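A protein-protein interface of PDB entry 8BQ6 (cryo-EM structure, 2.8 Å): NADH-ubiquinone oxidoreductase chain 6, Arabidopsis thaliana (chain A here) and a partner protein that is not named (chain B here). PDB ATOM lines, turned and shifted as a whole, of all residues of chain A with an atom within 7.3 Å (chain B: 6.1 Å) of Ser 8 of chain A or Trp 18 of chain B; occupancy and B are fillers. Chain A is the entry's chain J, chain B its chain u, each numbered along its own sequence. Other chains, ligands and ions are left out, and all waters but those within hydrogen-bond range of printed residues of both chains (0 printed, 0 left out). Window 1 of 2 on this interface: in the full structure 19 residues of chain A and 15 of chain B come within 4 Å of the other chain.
The backbone NH (N) of Ser 8 of chain A lies close to the indole nitrogen (NE1) of Trp 18 of chain B, at 3.5 Å.
The side-chain hydroxyl (OG) of Ser 4 of chain A sits at hydrogen-bond distance from the side-chain amide oxygen (OE1) of Gln 19 of chain B (2.9 Å).
OG of Ser 13 of chain A lies within hydrogen-bond range of OH of Tyr 7 of chain B, 2.6 Å away.
O of Ser 7 of chain A sits close to NE1 of Trp 18 of chain B (3.5 Å).
O of Leu 3 of chain A is in hydrogen-bond range of OG of Ser 7 of chain A (2.7 Å).
The backbone carbonyl oxygen (O) of Val 5 of chain A is in hydrogen-bond range of the side-chain hydroxyl (OG) of Ser 8 of chain A (2.9 Å).
The backbone carbonyl oxygen (O) of Leu 9 of chain A sits at hydrogen-bond distance from the side-chain hydroxyl (OG) of Ser 13 of chain A (3.1 Å).
The backbone carbonyl oxygen of Tyr 7 of chain B lies within hydrogen-bond range of the side-chain hydroxyl of Thr 11 of chain B.
OG of Ser 4 of chain A touches CB of Trp 18 of chain B, at 3.7 Å.
Ser 8 of chain A touches Thr 11 of chain B.
Ala 14 of chain B touches Ser 8 of chain A.
Ser 8 of chain A touches Phe 15 of chain B.
Leu 9 of chain A touches Thr 11 of chain B (CD2 to CG2, 3.7 Å).
Leu 11 of chain A touches Ala 14 of chain B (CD2 to CB, 3.9 Å).
Leu 11 of chain A touches Trp 18 of chain B (CD2 to NE1, 3.8 Å).
Val 12 of chain A touches Met 10 of chain B (CG2 to O, 3.6 Å).
CG2 of Val 12 of chain A touches N of Thr 11 of chain B (3.7 Å).
Met 21 of chain B touches Trp 98 of chain A (CE to NE1, 3.5 Å).
Ser 8 of chain A touches just these residues of chain B: Thr 11 (3.2 Å), Ala 14 (3.5 Å), Phe 15 (3.5 Å) and Trp 18 (3.5 Å).
Printed residues of chain A within 4 Å of Trp 18 of chain B: Ser 4, Ser 7, Ser 8 and Leu 11.
Of the printed residues of chain A, Gln 19 of chain B touches Ser 4 (2.9 Å).
Printed residues of chain B within 4 Å of Trp 98 of chain A: Met 21.
Printed residues of chain B within 4 Å of Ser 7 of chain A: Trp 18 (3.4 Å).
Of the printed residues of chain B, Val 5 of chain A touches Phe 15 (3.97 Å).
Of the printed residues of chain B, Leu 9 of chain A touches Tyr 7 and Thr 11.
The nearest residue of chain B that does not touch Ser 8 of chain A is Met 10 of chain B (5.6 Å).
The nearest printed residue of chain A that does not touch Phe 15 of chain B is Ile 2 of chain A (6.1 Å).
Hydrophobic or aromatic side chains of chain A within 4 Å of the printed part of chain B: Val 5, Leu 9, Leu 11, Val 12 and Trp 98.
Along chain A the printed residues that touch a printed residue of chain B span positions 4 to 98.
Hydrophobic or aromatic side chains of chain B within 4 Å of the printed part of chain A: Tyr 7, Met 10, Ala 14, Phe 15, Trp 18 and Met 21.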
ATOM      1  N   ILE A   2       0.539  18.879 -25.422  1.00  0.00           N
ATOM      2  CA  ILE A   2       1.165  18.250 -24.262  1.00  0.00           C
ATOM      3  C   ILE A   2       2.490  18.925 -23.951  1.00  0.00           C
ATOM      4  O   ILE A   2       2.827  19.172 -22.784  1.00  0.00           O
ATOM      5  CB  ILE A   2       1.352  16.743 -24.511  1.00  0.00           C
ATOM      6  CG1 ILE A   2       0.010  16.079 -24.810  1.00  0.00           C
ATOM      7  CG2 ILE A   2       2.042  16.090 -23.331  1.00  0.00           C
ATOM      8  CD1 ILE A   2       0.148  14.692 -25.389  1.00  0.00           C
ATOM      9  N   LEU A   3       3.273  19.217 -24.991  1.00  0.00           N
ATOM     10  CA  LEU A   3       4.500  19.971 -24.796  1.00  0.00           C
ATOM     11  C   LEU A   3       4.214  21.352 -24.231  1.00  0.00           C
ATOM     12  O   LEU A   3       5.009  21.868 -23.444  1.00  0.00           O
ATOM     13  CB  LEU A   3       5.275  20.078 -26.106  1.00  0.00           C
ATOM     14  CG  LEU A   3       5.894  18.791 -26.650  1.00  0.00           C
ATOM     15  CD1 LEU A   3       6.224  18.947 -28.127  1.00  0.00           C
ATOM     16  CD2 LEU A   3       7.127  18.417 -25.855  1.00  0.00           C
ATOM     17  N   SER A   4       3.073  21.949 -24.588  1.00  0.00           N
ATOM     18  CA  SER A   4       2.699  23.227 -23.994  1.00  0.00           C
ATOM     19  C   SER A   4       2.372  23.081 -22.512  1.00  0.00           C
ATOM     20  O   SER A   4       2.744  23.939 -21.705  1.00  0.00           O
ATOM     21  CB  SER A   4       1.520  23.838 -24.748  1.00  0.00           C
ATOM     22  OG  SER A   4       1.955  24.517 -25.911  1.00  0.00           O
ATOM     23  N   VAL A   5       1.683  22.004 -22.128  1.00  0.00           N
ATOM     24  CA  VAL A   5       1.375  21.802 -20.713  1.00  0.00           C
ATOM     25  C   VAL A   5       2.655  21.609 -19.914  1.00  0.00           C
ATOM     26  O   VAL A   5       2.847  22.226 -18.857  1.00  0.00           O
ATOM     27  CB  VAL A   5       0.420  20.611 -20.520  1.00  0.00           C
ATOM     28  CG1 VAL A   5       0.207  20.371 -19.039  1.00  0.00           C
ATOM     29  CG2 VAL A   5      -0.902  20.880 -21.196  1.00  0.00           C
ATOM     30  N   LEU A   6       3.544  20.742 -20.400  1.00  0.00           N
ATOM     31  CA  LEU A   6       4.795  20.522 -19.683  1.00  0.00           C
ATOM     32  C   LEU A   6       5.633  21.793 -19.643  1.00  0.00           C
ATOM     33  O   LEU A   6       6.227  22.118 -18.613  1.00  0.00           O
ATOM     34  CB  LEU A   6       5.581  19.375 -20.310  1.00  0.00           C
ATOM     35  CG  LEU A   6       4.960  17.982 -20.196  1.00  0.00           C
ATOM     36  CD1 LEU A   6       6.039  16.935 -20.362  1.00  0.00           C
ATOM     37  CD2 LEU A   6       4.198  17.782 -18.889  1.00  0.00           C
ATOM     38  N   SER A   7       5.679  22.540 -20.742  1.00  0.00           N
ATOM     39  CA  SER A   7       6.443  23.779 -20.737  1.00  0.00           C
ATOM     40  C   SER A   7       5.885  24.769 -19.725  1.00  0.00           C
ATOM     41  O   SER A   7       6.646  25.430 -19.018  1.00  0.00           O
ATOM     42  CB  SER A   7       6.456  24.389 -22.136  1.00  0.00           C
ATOM     43  OG  SER A   7       7.095  23.526 -23.058  1.00  0.00           O
ATOM     44  N   SER A   8       4.558  24.881 -19.640  1.00  0.00           N
ATOM     45  CA  SER A   8       3.950  25.794 -18.679  1.00  0.00           C
ATOM     46  C   SER A   8       4.219  25.360 -17.241  1.00  0.00           C
ATOM     47  O   SER A   8       4.519  26.197 -16.377  1.00  0.00           O
ATOM     48  CB  SER A   8       2.452  25.893 -18.948  1.00  0.00           C
ATOM     49  OG  SER A   8       1.751  24.876 -18.263  1.00  0.00           O
ATOM     50  N   LEU A   9       4.115  24.059 -16.963  1.00  0.00           N
ATOM     51  CA  LEU A   9       4.420  23.582 -15.618  1.00  0.00           C
ATOM     52  C   LEU A   9       5.869  23.872 -15.254  1.00  0.00           C
ATOM     53  O   LEU A   9       6.155  24.369 -14.158  1.00  0.00           O
ATOM     54  CB  LEU A   9       4.124  22.089 -15.498  1.00  0.00           C
ATOM     55  CG  LEU A   9       2.642  21.726 -15.394  1.00  0.00           C
ATOM     56  CD1 LEU A   9       2.452  20.218 -15.344  1.00  0.00           C
ATOM     57  CD2 LEU A   9       2.000  22.399 -14.185  1.00  0.00           C
ATOM     58  N   ALA A  10       6.794  23.598 -16.175  1.00  0.00           N
ATOM     59  CA  ALA A  10       8.204  23.851 -15.903  1.00  0.00           C
ATOM     60  C   ALA A  10       8.482  25.338 -15.743  1.00  0.00           C
ATOM     61  O   ALA A  10       9.307  25.732 -14.916  1.00  0.00           O
ATOM     62  CB  ALA A  10       9.067  23.257 -17.012  1.00  0.00           C
ATOM     63  N   LEU A  11       7.801  26.182 -16.519  1.00  0.00           N
ATOM     64  CA  LEU A  11       8.018  27.622 -16.423  1.00  0.00           C
ATOM     65  C   LEU A  11       7.561  28.159 -15.073  1.00  0.00           C
ATOM     66  O   LEU A  11       8.277  28.932 -14.422  1.00  0.00           O
ATOM     67  CB  LEU A  11       7.290  28.329 -17.565  1.00  0.00           C
ATOM     68  CG  LEU A  11       7.149  29.851 -17.570  1.00  0.00           C
ATOM     69  CD1 LEU A  11       8.466  30.559 -17.312  1.00  0.00           C
ATOM     70  CD2 LEU A  11       6.559  30.286 -18.894  1.00  0.00           C
ATOM     71  N   VAL A  12       6.370  27.756 -14.628  1.00  0.00           N
ATOM     72  CA  VAL A  12       5.902  28.214 -13.325  1.00  0.00           C
ATOM     73  C   VAL A  12       6.796  27.673 -12.215  1.00  0.00           C
ATOM     74  O   VAL A  12       7.190  28.409 -11.299  1.00  0.00           O
ATOM     75  CB  VAL A  12       4.429  27.828 -13.120  1.00  0.00           C
ATOM     76  CG1 VAL A  12       3.916  28.405 -11.826  1.00  0.00           C
ATOM     77  CG2 VAL A  12       3.597  28.341 -14.266  1.00  0.00           C
ATOM     78  N   SER A  13       7.153  26.388 -12.288  1.00  0.00           N
ATOM     79  CA  SER A  13       7.959  25.783 -11.233  1.00  0.00           C
ATOM     80  C   SER A  13       9.346  26.413 -11.171  1.00  0.00           C
ATOM     81  O   SER A  13       9.902  26.602 -10.083  1.00  0.00           O
ATOM     82  CB  SER A  13       8.051  24.277 -11.460  1.00  0.00           C
ATOM     83  OG  SER A  13       6.816  23.649 -11.176  1.00  0.00           O
ATOM     84  N   GLY A  14       9.920  26.756 -12.326  1.00  0.00           N
ATOM     85  CA  GLY A  14      11.200  27.442 -12.334  1.00  0.00           C
ATOM     86  C   GLY A  14      11.115  28.852 -11.785  1.00  0.00           C
ATOM     87  O   GLY A  14      12.010  29.302 -11.059  1.00  0.00           O
ATOM     88  N   LEU A  15      10.045  29.578 -12.125  1.00  0.00           N
ATOM     89  CA  LEU A  15       9.863  30.890 -11.521  1.00  0.00           C
ATOM     90  C   LEU A  15       9.801  30.773 -10.009  1.00  0.00           C
ATOM     91  O   LEU A  15      10.371  31.598  -9.288  1.00  0.00           O
ATOM     92  CB  LEU A  15       8.598  31.551 -12.049  1.00  0.00           C
ATOM     93  CG  LEU A  15       8.657  32.011 -13.496  1.00  0.00           C
ATOM     94  CD1 LEU A  15       7.247  32.220 -13.981  1.00  0.00           C
ATOM     95  CD2 LEU A  15       9.474  33.284 -13.627  1.00  0.00           C
ATOM     96  N   ASP A  36       9.112  17.369 -14.310  1.00  0.00           N
ATOM     97  CA  ASP A  36       8.620  17.778 -15.622  1.00  0.00           C
ATOM     98  C   ASP A  36       9.619  17.450 -16.729  1.00  0.00           C
ATOM     99  O   ASP A  36       9.239  17.024 -17.834  1.00  0.00           O
ATOM    100  CB  ASP A  36       8.308  19.266 -15.586  1.00  0.00           C
ATOM    101  CG  ASP A  36       7.148  19.615 -16.442  1.00  0.00           C
ATOM    102  OD1 ASP A  36       7.020  20.792 -16.787  1.00  0.00           O
ATOM    103  OD2 ASP A  36       6.386  18.694 -16.795  1.00  0.00           O
ATOM    104  N   TRP A  98      15.721  36.170 -25.471  1.00  0.00           N
ATOM    105  CA  TRP A  98      14.541  35.582 -26.094  1.00  0.00           C
ATOM    106  C   TRP A  98      14.590  35.737 -27.605  1.00  0.00           C
ATOM    107  O   TRP A  98      14.640  34.744 -28.340  1.00  0.00           O
ATOM    108  CB  TRP A  98      13.283  36.240 -25.518  1.00  0.00           C
ATOM    109  CG  TRP A  98      11.987  35.797 -26.138  1.00  0.00           C
ATOM    110  CD1 TRP A  98      11.330  34.625 -25.914  1.00  0.00           C
ATOM    111  CD2 TRP A  98      11.178  36.539 -27.062  1.00  0.00           C
ATOM    112  NE1 TRP A  98      10.171  34.581 -26.651  1.00  0.00           N
ATOM    113  CE2 TRP A  98      10.054  35.745 -27.363  1.00  0.00           C
ATOM    114  CE3 TRP A  98      11.297  37.794 -27.665  1.00  0.00           C
ATOM    115  CZ2 TRP A  98       9.059  36.164 -28.244  1.00  0.00           C
ATOM    116  CZ3 TRP A  98      10.309  38.206 -28.539  1.00  0.00           C
ATOM    117  CH2 TRP A  98       9.203  37.395 -28.819  1.00  0.00           C
ATOM    118  N   PHE A 102      15.438  31.953 -28.574  1.00  0.00           N
ATOM    119  CA  PHE A 102      14.242  31.158 -28.805  1.00  0.00           C
ATOM    120  C   PHE A 102      14.018  30.909 -30.287  1.00  0.00           C
ATOM    121  O   PHE A 102      13.184  30.073 -30.647  1.00  0.00           O
ATOM    122  CB  PHE A 102      13.007  31.843 -28.215  1.00  0.00           C
ATOM    123  CG  PHE A 102      12.933  31.775 -26.722  1.00  0.00           C
ATOM    124  CD1 PHE A 102      13.982  32.220 -25.942  1.00  0.00           C
ATOM    125  CD2 PHE A 102      11.816  31.257 -26.096  1.00  0.00           C
ATOM    126  CE1 PHE A 102      13.916  32.163 -24.576  1.00  0.00           C
ATOM    127  CE2 PHE A 102      11.749  31.193 -24.726  1.00  0.00           C
ATOM    128  CZ  PHE A 102      12.801  31.647 -23.967  1.00  0.00           C
ATOM    129  N   TYR B   7      -0.917  29.179  -8.171  1.00  0.00           N
ATOM    130  CA  TYR B   7      -0.088  28.330  -9.022  1.00  0.00           C
ATOM    131  C   TYR B   7      -0.867  27.861 -10.253  1.00  0.00           C
ATOM    132  O   TYR B   7      -0.329  27.840 -11.369  1.00  0.00           O
ATOM    133  CB  TYR B   7       0.458  27.153  -8.209  1.00  0.00           C
ATOM    134  CG  TYR B   7       1.497  26.333  -8.933  1.00  0.00           C
ATOM    135  CD1 TYR B   7       1.119  25.292  -9.761  1.00  0.00           C
ATOM    136  CD2 TYR B   7       2.854  26.606  -8.799  1.00  0.00           C
ATOM    137  CE1 TYR B   7       2.047  24.542 -10.428  1.00  0.00           C
ATOM    138  CE2 TYR B   7       3.799  25.852  -9.469  1.00  0.00           C
ATOM    139  CZ  TYR B   7       3.382  24.822 -10.283  1.00  0.00           C
ATOM    140  OH  TYR B   7       4.292  24.056 -10.965  1.00  0.00           O
ATOM    141  N   MET B  10      -1.147  30.876 -12.676  1.00  0.00           N
ATOM    142  CA  MET B  10       0.111  31.110 -13.373  1.00  0.00           C
ATOM    143  C   MET B  10       0.350  30.044 -14.431  1.00  0.00           C
ATOM    144  O   MET B  10       0.883  30.340 -15.508  1.00  0.00           O
ATOM    145  CB  MET B  10       1.270  31.175 -12.386  1.00  0.00           C
ATOM    146  CG  MET B  10       1.415  32.537 -11.747  1.00  0.00           C
ATOM    147  SD  MET B  10       2.953  32.719 -10.840  1.00  0.00           S
ATOM    148  CE  MET B  10       2.661  31.618  -9.462  1.00  0.00           C
ATOM    149  N   THR B  11      -0.061  28.802 -14.160  1.00  0.00           N
ATOM    150  CA  THR B  11       0.047  27.765 -15.183  1.00  0.00           C
ATOM    151  C   THR B  11      -0.833  28.067 -16.390  1.00  0.00           C
ATOM    152  O   THR B  11      -0.416  27.858 -17.534  1.00  0.00           O
ATOM    153  CB  THR B  11      -0.317  26.402 -14.612  1.00  0.00           C
ATOM    154  OG1 THR B  11       0.341  26.215 -13.354  1.00  0.00           O
ATOM    155  CG2 THR B  11       0.119  25.322 -15.571  1.00  0.00           C
ATOM    156  N   LEU B  12      -2.065  28.521 -16.157  1.00  0.00           N
ATOM    157  CA  LEU B  12      -2.934  28.880 -17.277  1.00  0.00           C
ATOM    158  C   LEU B  12      -2.310  29.975 -18.125  1.00  0.00           C
ATOM    159  O   LEU B  12      -2.308  29.902 -19.364  1.00  0.00           O
ATOM    160  CB  LEU B  12      -4.287  29.354 -16.770  1.00  0.00           C
ATOM    161  CG  LEU B  12      -5.258  28.294 -16.301  1.00  0.00           C
ATOM    162  CD1 LEU B  12      -6.475  28.999 -15.750  1.00  0.00           C
ATOM    163  CD2 LEU B  12      -5.614  27.403 -17.462  1.00  0.00           C
ATOM    164  N   ALA B  13      -1.782  31.004 -17.465  1.00  0.00           N
ATOM    165  CA  ALA B  13      -1.126  32.083 -18.189  1.00  0.00           C
ATOM    166  C   ALA B  13       0.073  31.569 -18.979  1.00  0.00           C
ATOM    167  O   ALA B  13       0.306  31.992 -20.118  1.00  0.00           O
ATOM    168  CB  ALA B  13      -0.707  33.181 -17.212  1.00  0.00           C
ATOM    169  N   ALA B  14       0.846  30.652 -18.396  1.00  0.00           N
ATOM    170  CA  ALA B  14       1.987  30.098 -19.117  1.00  0.00           C
ATOM    171  C   ALA B  14       1.538  29.280 -20.325  1.00  0.00           C
ATOM    172  O   ALA B  14       2.170  29.323 -21.386  1.00  0.00           O
ATOM    173  CB  ALA B  14       2.842  29.259 -18.169  1.00  0.00           C
ATOM    174  N   PHE B  15       0.445  28.530 -20.181  1.00  0.00           N
ATOM    175  CA  PHE B  15      -0.095  27.780 -21.310  1.00  0.00           C
ATOM    176  C   PHE B  15      -0.475  28.719 -22.451  1.00  0.00           C
ATOM    177  O   PHE B  15      -0.164  28.454 -23.625  1.00  0.00           O
ATOM    178  CB  PHE B  15      -1.297  26.955 -20.851  1.00  0.00           C
ATOM    179  CG  PHE B  15      -1.859  26.060 -21.911  1.00  0.00           C
ATOM    180  CD1 PHE B  15      -1.157  24.953 -22.352  1.00  0.00           C
ATOM    181  CD2 PHE B  15      -3.087  26.335 -22.477  1.00  0.00           C
ATOM    182  CE1 PHE B  15      -1.677  24.135 -23.333  1.00  0.00           C
ATOM    183  CE2 PHE B  15      -3.607  25.523 -23.457  1.00  0.00           C
ATOM    184  CZ  PHE B  15      -2.901  24.421 -23.887  1.00  0.00           C
ATOM    185  N   ALA B  16      -1.119  29.842 -22.118  1.00  0.00           N
ATOM    186  CA  ALA B  16      -1.433  30.844 -23.134  1.00  0.00           C
ATOM    187  C   ALA B  16      -0.167  31.397 -23.780  1.00  0.00           C
ATOM    188  O   ALA B  16      -0.121  31.612 -25.000  1.00  0.00           O
ATOM    189  CB  ALA B  16      -2.255  31.977 -22.522  1.00  0.00           C
ATOM    190  N   PHE B  17       0.871  31.640 -22.976  1.00  0.00           N
ATOM    191  CA  PHE B  17       2.122  32.148 -23.530  1.00  0.00           C
ATOM    192  C   PHE B  17       2.712  31.170 -24.543  1.00  0.00           C
ATOM    193  O   PHE B  17       3.200  31.577 -25.605  1.00  0.00           O
ATOM    194  CB  PHE B  17       3.119  32.434 -22.406  1.00  0.00           C
ATOM    195  CG  PHE B  17       4.549  32.497 -22.863  1.00  0.00           C
ATOM    196  CD1 PHE B  17       5.049  33.653 -23.439  1.00  0.00           C
ATOM    197  CD2 PHE B  17       5.399  31.415 -22.702  1.00  0.00           C
ATOM    198  CE1 PHE B  17       6.361  33.723 -23.863  1.00  0.00           C
ATOM    199  CE2 PHE B  17       6.712  31.480 -23.124  1.00  0.00           C
ATOM    200  CZ  PHE B  17       7.195  32.638 -23.704  1.00  0.00           C
ATOM    201  N   TRP B  18       2.662  29.875 -24.235  1.00  0.00           N
ATOM    202  CA  TRP B  18       3.259  28.889 -25.134  1.00  0.00           C
ATOM    203  C   TRP B  18       2.459  28.748 -26.426  1.00  0.00           C
ATOM    204  O   TRP B  18       3.038  28.562 -27.505  1.00  0.00           O
ATOM    205  CB  TRP B  18       3.404  27.554 -24.413  1.00  0.00           C
ATOM    206  CG  TRP B  18       4.493  27.620 -23.407  1.00  0.00           C
ATOM    207  CD1 TRP B  18       4.362  27.573 -22.056  1.00  0.00           C
ATOM    208  CD2 TRP B  18       5.890  27.780 -23.671  1.00  0.00           C
ATOM    209  NE1 TRP B  18       5.589  27.687 -21.457  1.00  0.00           N
ATOM    210  CE2 TRP B  18       6.546  27.814 -22.429  1.00  0.00           C
ATOM    211  CE3 TRP B  18       6.651  27.891 -24.839  1.00  0.00           C
ATOM    212  CZ2 TRP B  18       7.925  27.950 -22.316  1.00  0.00           C
ATOM    213  CZ3 TRP B  18       8.021  28.028 -24.725  1.00  0.00           C
ATOM    214  CH2 TRP B  18       8.644  28.055 -23.474  1.00  0.00           C
ATOM    215  N   GLN B  19       1.131  28.857 -26.348  1.00  0.00           N
ATOM    216  CA  GLN B  19       0.345  28.858 -27.583  1.00  0.00           C
ATOM    217  C   GLN B  19       0.649  30.095 -28.439  1.00  0.00           C
ATOM    218  O   GLN B  19       0.706  30.015 -29.680  1.00  0.00           O
ATOM    219  CB  GLN B  19      -1.143  28.759 -27.254  1.00  0.00           C
ATOM    220  CG  GLN B  19      -1.494  27.601 -26.319  1.00  0.00           C
ATOM    221  CD  GLN B  19      -1.392  26.232 -26.976  1.00  0.00           C
ATOM    222  OE1 GLN B  19      -0.300  25.748 -27.272  1.00  0.00           O
ATOM    223  NE2 GLN B  19      -2.535  25.590 -27.185  1.00  0.00           N
ATOM    224  N   SER B  20       0.860  31.247 -27.794  1.00  0.00           N
ATOM    225  CA  SER B  20       1.279  32.430 -28.545  1.00  0.00           C
ATOM    226  C   SER B  20       2.621  32.201 -29.230  1.00  0.00           C
ATOM    227  O   SER B  20       2.823  32.610 -30.382  1.00  0.00           O
ATOM    228  CB  SER B  20       1.352  33.648 -27.626  1.00  0.00           C
ATOM    229  OG  SER B  20       0.262  33.682 -26.725  1.00  0.00           O
ATOM    230  N   MET B  21       3.554  31.556 -28.528  1.00  0.00           N
ATOM    231  CA  MET B  21       4.836  31.217 -29.137  1.00  0.00           C
ATOM    232  C   MET B  21       4.653  30.299 -30.340  1.00  0.00           C
ATOM    233  O   MET B  21       5.393  30.400 -31.326  1.00  0.00           O
ATOM    234  CB  MET B  21       5.748  30.568 -28.099  1.00  0.00           C
ATOM    235  CG  MET B  21       6.357  31.549 -27.119  1.00  0.00           C
ATOM    236  SD  MET B  21       6.783  33.124 -27.880  1.00  0.00           S
ATOM    237  CE  MET B  21       8.224  32.644 -28.826  1.00  0.00           C
ATOM    238  N   ASP B  22       3.675  29.393 -30.278  1.00  0.00           N
ATOM    239  CA  ASP B  22       3.377  28.556 -31.440  1.00  0.00           C
ATOM    240  C   ASP B  22       2.969  29.409 -32.636  1.00  0.00           C
ATOM    241  O   ASP B  22       3.412  29.179 -33.773  1.00  0.00           O
ATOM    242  CB  ASP B  22       2.272  27.555 -31.103  1.00  0.00           C
ATOM    243  CG  ASP B  22       2.797  26.320 -30.408  1.00  0.00           C
ATOM    244  OD1 ASP B  22       3.694  26.451 -29.549  1.00  0.00           O
ATOM    245  OD2 ASP B  22       2.318  25.212 -30.731  1.00  0.00           O
ATOM    246  N   LYS B  23       2.118  30.408 -32.392  1.00  0.00           N
ATOM    247  CA  LYS B  23       1.724  31.308 -33.476  1.00  0.00           C
ATOM    248  C   LYS B  23       2.923  32.070 -34.035  1.00  0.00           C
ATOM    249  O   LYS B  23       3.034  32.267 -35.253  1.00  0.00           O
ATOM    250  CB  LYS B  23       0.649  32.274 -32.990  1.00  0.00           C
ATOM    251  CG  LYS B  23      -0.565  31.564 -32.443  1.00  0.00           C
ATOM    252  CD  LYS B  23      -1.786  32.455 -32.439  1.00  0.00           C
ATOM    253  CE  LYS B  23      -3.038  31.630 -32.187  1.00  0.00           C
ATOM    254  NZ  LYS B  23      -3.370  31.525 -30.738  1.00  0.00           N
